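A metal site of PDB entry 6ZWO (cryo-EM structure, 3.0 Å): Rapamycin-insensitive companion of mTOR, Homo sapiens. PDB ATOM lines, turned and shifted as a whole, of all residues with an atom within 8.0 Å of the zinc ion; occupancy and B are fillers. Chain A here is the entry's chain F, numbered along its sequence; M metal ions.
SG of Cys 1520 lies close to N of Tyr 1522. The side-chain sulfur (SG) of Cys 1520 sits close to the side-chain hydroxyl (OG) of Ser 1654, 3.7 Å away.
Of the 19 residues printed, 4 come within 4 Å of the zinc ion. The nearest printed residue that does not touch the zinc ion is Thr 1516 (4.9 Å).
The zinc ion is bound by a ring nitrogen (NE2) of His 1515 (2.2 Å), the side-chain sulfur of Cys 1520 (2.3 Å), the side-chain sulfur of Cys 1523 (2.3 Å) and the side-chain sulfur of Cys 1651 (2.4 Å). The zinc ion has four donor atoms within binding distance.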
ATOM      1  N   LEU A1512      -4.460 -24.555 -28.876  1.00  0.00           N
ATOM      2  CA  LEU A1512      -5.382 -23.444 -28.981  1.00  0.00           C
ATOM      3  C   LEU A1512      -5.506 -23.044 -30.445  1.00  0.00           C
ATOM      4  O   LEU A1512      -4.511 -22.682 -31.081  1.00  0.00           O
ATOM      5  CB  LEU A1512      -4.892 -22.265 -28.137  1.00  0.00           C
ATOM      6  CG  LEU A1512      -4.555 -22.577 -26.688  1.00  0.00           C
ATOM      7  CD1 LEU A1512      -3.687 -21.500 -26.082  1.00  0.00           C
ATOM      8  CD2 LEU A1512      -5.835 -22.760 -25.875  1.00  0.00           C
ATOM      9  N   HIS A1515      -6.024 -18.564 -30.981  1.00  0.00           N
ATOM     10  CA  HIS A1515      -5.266 -17.824 -29.980  1.00  0.00           C
ATOM     11  C   HIS A1515      -4.163 -17.044 -30.671  1.00  0.00           C
ATOM     12  O   HIS A1515      -3.353 -17.620 -31.405  1.00  0.00           O
ATOM     13  CB  HIS A1515      -4.680 -18.760 -28.919  1.00  0.00           C
ATOM     14  CG  HIS A1515      -3.693 -18.091 -28.002  1.00  0.00           C
ATOM     15  ND1 HIS A1515      -2.421 -17.739 -28.409  1.00  0.00           N
ATOM     16  CD2 HIS A1515      -3.812 -17.673 -26.727  1.00  0.00           C
ATOM     17  CE1 HIS A1515      -1.794 -17.138 -27.419  1.00  0.00           C
ATOM     18  NE2 HIS A1515      -2.615 -17.085 -26.386  1.00  0.00           N
ATOM     19  N   THR A1516      -4.155 -15.726 -30.460  1.00  0.00           N
ATOM     20  CA  THR A1516      -3.134 -14.836 -30.987  1.00  0.00           C
ATOM     21  C   THR A1516      -2.658 -13.946 -29.845  1.00  0.00           C
ATOM     22  O   THR A1516      -3.141 -14.033 -28.715  1.00  0.00           O
ATOM     23  CB  THR A1516      -3.685 -14.012 -32.165  1.00  0.00           C
ATOM     24  OG1 THR A1516      -4.558 -14.829 -32.946  1.00  0.00           O
ATOM     25  CG2 THR A1516      -2.555 -13.527 -33.068  1.00  0.00           C
ATOM     26  N   ASP A1517      -1.662 -13.094 -30.130  1.00  0.00           N
ATOM     27  CA  ASP A1517      -1.206 -12.135 -29.139  1.00  0.00           C
ATOM     28  C   ASP A1517      -2.357 -11.230 -28.703  1.00  0.00           C
ATOM     29  O   ASP A1517      -2.555 -11.004 -27.508  1.00  0.00           O
ATOM     30  CB  ASP A1517      -0.053 -11.307 -29.696  1.00  0.00           C
ATOM     31  CG  ASP A1517       1.296 -11.952 -29.442  1.00  0.00           C
ATOM     32  OD1 ASP A1517       1.335 -13.027 -28.820  1.00  0.00           O
ATOM     33  OD2 ASP A1517       2.325 -11.375 -29.877  1.00  0.00           O
ATOM     34  N   ASP A1518      -3.107 -10.703 -29.662  1.00  0.00           N
ATOM     35  CA  ASP A1518      -4.351 -10.026 -29.354  1.00  0.00           C
ATOM     36  C   ASP A1518      -5.447 -11.066 -29.093  1.00  0.00           C
ATOM     37  O   ASP A1518      -5.371 -12.193 -29.584  1.00  0.00           O
ATOM     38  CB  ASP A1518      -4.758  -9.109 -30.503  1.00  0.00           C
ATOM     39  CG  ASP A1518      -6.123  -8.467 -30.292  1.00  0.00           C
ATOM     40  OD1 ASP A1518      -6.207  -7.495 -29.505  1.00  0.00           O
ATOM     41  OD2 ASP A1518      -7.100  -8.928 -30.906  1.00  0.00           O
ATOM     42  N   ASN A1519      -6.423 -10.675 -28.279  1.00  0.00           N
ATOM     43  CA  ASN A1519      -7.567 -11.472 -27.817  1.00  0.00           C
ATOM     44  C   ASN A1519      -7.185 -12.489 -26.750  1.00  0.00           C
ATOM     45  O   ASN A1519      -7.960 -13.412 -26.460  1.00  0.00           O
ATOM     46  CB  ASN A1519      -8.361 -12.120 -28.986  1.00  0.00           C
ATOM     47  CG  ASN A1519      -7.836 -13.500 -29.445  1.00  0.00           C
ATOM     48  OD1 ASN A1519      -6.991 -14.145 -28.826  1.00  0.00           O
ATOM     49  ND2 ASN A1519      -8.379 -13.949 -30.570  1.00  0.00           N
ATOM     50  N   CYS A1520      -6.020 -12.329 -26.138  1.00  0.00           N
ATOM     51  CA  CYS A1520      -5.614 -13.138 -24.998  1.00  0.00           C
ATOM     52  C   CYS A1520      -5.455 -12.236 -23.784  1.00  0.00           C
ATOM     53  O   CYS A1520      -4.907 -11.136 -23.887  1.00  0.00           O
ATOM     54  CB  CYS A1520      -4.306 -13.888 -25.260  1.00  0.00           C
ATOM     55  SG  CYS A1520      -3.700 -14.799 -23.815  1.00  0.00           S
ATOM     56  N   LEU A1521      -5.946 -12.703 -22.630  1.00  0.00           N
ATOM     57  CA  LEU A1521      -5.955 -11.868 -21.434  1.00  0.00           C
ATOM     58  C   LEU A1521      -4.547 -11.456 -21.027  1.00  0.00           C
ATOM     59  O   LEU A1521      -4.335 -10.335 -20.548  1.00  0.00           O
ATOM     60  CB  LEU A1521      -6.640 -12.624 -20.291  1.00  0.00           C
ATOM     61  CG  LEU A1521      -8.140 -12.373 -20.099  1.00  0.00           C
ATOM     62  CD1 LEU A1521      -8.825 -13.617 -19.568  1.00  0.00           C
ATOM     63  CD2 LEU A1521      -8.371 -11.199 -19.178  1.00  0.00           C
ATOM     64  N   TYR A1522      -3.562 -12.337 -21.211  1.00  0.00           N
ATOM     65  CA  TYR A1522      -2.196 -12.054 -20.787  1.00  0.00           C
ATOM     66  C   TYR A1522      -1.304 -11.610 -21.936  1.00  0.00           C
ATOM     67  O   TYR A1522      -0.500 -10.687 -21.784  1.00  0.00           O
ATOM     68  CB  TYR A1522      -1.602 -13.285 -20.089  1.00  0.00           C
ATOM     69  CG  TYR A1522      -0.192 -13.129 -19.568  1.00  0.00           C
ATOM     70  CD1 TYR A1522       0.044 -13.032 -18.204  1.00  0.00           C
ATOM     71  CD2 TYR A1522       0.906 -13.157 -20.414  1.00  0.00           C
ATOM     72  CE1 TYR A1522       1.322 -12.898 -17.707  1.00  0.00           C
ATOM     73  CE2 TYR A1522       2.198 -13.030 -19.932  1.00  0.00           C
ATOM     74  CZ  TYR A1522       2.391 -12.914 -18.570  1.00  0.00           C
ATOM     75  OH  TYR A1522       3.670 -12.789 -18.068  1.00  0.00           O
ATOM     76  N   CYS A1523      -1.433 -12.253 -23.107  1.00  0.00           N
ATOM     77  CA  CYS A1523      -0.463 -12.044 -24.179  1.00  0.00           C
ATOM     78  C   CYS A1523      -0.492 -10.606 -24.705  1.00  0.00           C
ATOM     79  O   CYS A1523       0.520 -10.121 -25.232  1.00  0.00           O
ATOM     80  CB  CYS A1523      -0.706 -13.042 -25.301  1.00  0.00           C
ATOM     81  SG  CYS A1523      -0.210 -14.745 -24.905  1.00  0.00           S
ATOM     82  N   VAL A1524      -1.633  -9.931 -24.595  1.00  0.00           N
ATOM     83  CA  VAL A1524      -1.708  -8.543 -25.059  1.00  0.00           C
ATOM     84  C   VAL A1524      -0.747  -7.643 -24.305  1.00  0.00           C
ATOM     85  O   VAL A1524      -0.265  -6.638 -24.856  1.00  0.00           O
ATOM     86  CB  VAL A1524      -3.158  -8.013 -24.968  1.00  0.00           C
ATOM     87  CG1 VAL A1524      -4.088  -8.831 -25.831  1.00  0.00           C
ATOM     88  CG2 VAL A1524      -3.633  -8.038 -23.517  1.00  0.00           C
ATOM     89  N   ILE A1526       2.315  -8.265 -23.148  1.00  0.00           N
ATOM     90  CA  ILE A1526       3.757  -8.481 -23.306  1.00  0.00           C
ATOM     91  C   ILE A1526       4.385  -7.407 -24.186  1.00  0.00           C
ATOM     92  O   ILE A1526       5.528  -6.988 -23.950  1.00  0.00           O
ATOM     93  CB  ILE A1526       4.031  -9.902 -23.831  1.00  0.00           C
ATOM     94  CG1 ILE A1526       3.716 -10.018 -25.332  1.00  0.00           C
ATOM     95  CG2 ILE A1526       3.235 -10.920 -23.035  1.00  0.00           C
ATOM     96  CD1 ILE A1526       3.796 -11.430 -25.855  1.00  0.00           C
ATOM     97  N   SER A1534       5.194 -15.947 -21.282  1.00  0.00           N
ATOM     98  CA  SER A1534       4.590 -17.039 -20.551  1.00  0.00           C
ATOM     99  C   SER A1534       5.586 -18.167 -20.312  1.00  0.00           C
ATOM    100  O   SER A1534       6.429 -18.463 -21.162  1.00  0.00           O
ATOM    101  CB  SER A1534       3.372 -17.577 -21.304  1.00  0.00           C
ATOM    102  OG  SER A1534       3.644 -17.716 -22.692  1.00  0.00           O
ATOM    103  N   ARG A1613      -5.345 -29.827 -23.340  1.00  0.00           N
ATOM    104  CA  ARG A1613      -5.819 -28.509 -23.748  1.00  0.00           C
ATOM    105  C   ARG A1613      -6.859 -28.622 -24.864  1.00  0.00           C
ATOM    106  O   ARG A1613      -7.996 -28.148 -24.733  1.00  0.00           O
ATOM    107  CB  ARG A1613      -4.627 -27.654 -24.190  1.00  0.00           C
ATOM    108  CG  ARG A1613      -4.955 -26.203 -24.468  1.00  0.00           C
ATOM    109  CD  ARG A1613      -3.673 -25.385 -24.551  1.00  0.00           C
ATOM    110  NE  ARG A1613      -3.143 -25.053 -23.233  1.00  0.00           N
ATOM    111  CZ  ARG A1613      -2.216 -24.124 -23.020  1.00  0.00           C
ATOM    112  NH1 ARG A1613      -1.717 -23.432 -24.040  1.00  0.00           N
ATOM    113  NH2 ARG A1613      -1.779 -23.880 -21.796  1.00  0.00           N
ATOM    114  N   ILE A1650      -3.794 -19.457 -17.979  1.00  0.00           N
ATOM    115  CA  ILE A1650      -4.707 -18.383 -18.315  1.00  0.00           C
ATOM    116  C   ILE A1650      -4.820 -18.252 -19.824  1.00  0.00           C
ATOM    117  O   ILE A1650      -5.771 -17.654 -20.343  1.00  0.00           O
ATOM    118  CB  ILE A1650      -4.248 -17.060 -17.670  1.00  0.00           C
ATOM    119  CG1 ILE A1650      -5.283 -15.951 -17.918  1.00  0.00           C
ATOM    120  CG2 ILE A1650      -2.892 -16.646 -18.212  1.00  0.00           C
ATOM    121  CD1 ILE A1650      -4.799 -14.581 -17.519  1.00  0.00           C
ATOM    122  N   CYS A1651      -3.894 -18.864 -20.557  1.00  0.00           N
ATOM    123  CA  CYS A1651      -3.978 -18.869 -22.006  1.00  0.00           C
ATOM    124  C   CYS A1651      -5.018 -19.860 -22.526  1.00  0.00           C
ATOM    125  O   CYS A1651      -5.312 -19.845 -23.725  1.00  0.00           O
ATOM    126  CB  CYS A1651      -2.619 -19.180 -22.628  1.00  0.00           C
ATOM    127  SG  CYS A1651      -1.519 -17.753 -22.791  1.00  0.00           S
ATOM    128  N   LEU A1652      -5.563 -20.697 -21.653  1.00  0.00           N
ATOM    129  CA  LEU A1652      -6.722 -21.522 -21.959  1.00  0.00           C
ATOM    130  C   LEU A1652      -8.017 -20.873 -21.500  1.00  0.00           C
ATOM    131  O   LEU A1652      -9.043 -21.003 -22.182  1.00  0.00           O
ATOM    132  CB  LEU A1652      -6.576 -22.896 -21.301  1.00  0.00           C
ATOM    133  CG  LEU A1652      -7.775 -23.850 -21.345  1.00  0.00           C
ATOM    134  CD1 LEU A1652      -8.176 -24.134 -22.787  1.00  0.00           C
ATOM    135  CD2 LEU A1652      -7.459 -25.143 -20.616  1.00  0.00           C
ATOM    136  N   SER A1654      -8.444 -17.680 -21.486  1.00  0.00           N
ATOM    137  CA  SER A1654      -8.658 -16.686 -22.535  1.00  0.00           C
ATOM    138  C   SER A1654      -9.335 -17.313 -23.746  1.00  0.00           C
ATOM    139  O   SER A1654     -10.258 -16.720 -24.325  1.00  0.00           O
ATOM    140  CB  SER A1654      -7.331 -16.043 -22.928  1.00  0.00           C
ATOM    141  OG  SER A1654      -6.668 -15.535 -21.793  1.00  0.00           O
ATOM    142  N   GLU A1655      -8.909 -18.516 -24.130  1.00  0.00           N
ATOM    143  CA  GLU A1655      -9.495 -19.178 -25.292  1.00  0.00           C
ATOM    144  C   GLU A1655     -10.954 -19.555 -25.041  1.00  0.00           C
ATOM    145  O   GLU A1655     -11.814 -19.336 -25.904  1.00  0.00           O
ATOM    146  CB  GLU A1655      -8.676 -20.412 -25.663  1.00  0.00           C
ATOM    147  CG  GLU A1655      -9.186 -21.152 -26.881  1.00  0.00           C
ATOM    148  CD  GLU A1655      -8.845 -20.466 -28.179  1.00  0.00           C
ATOM    149  OE1 GLU A1655      -7.915 -19.618 -28.171  1.00  0.00           O
ATOM    150  OE2 GLU A1655      -9.490 -20.760 -29.204  1.00  0.00           O
HETATM  151 ZN    ZN M   1      -1.989 -16.141 -24.445  1.00  0.00          ZN
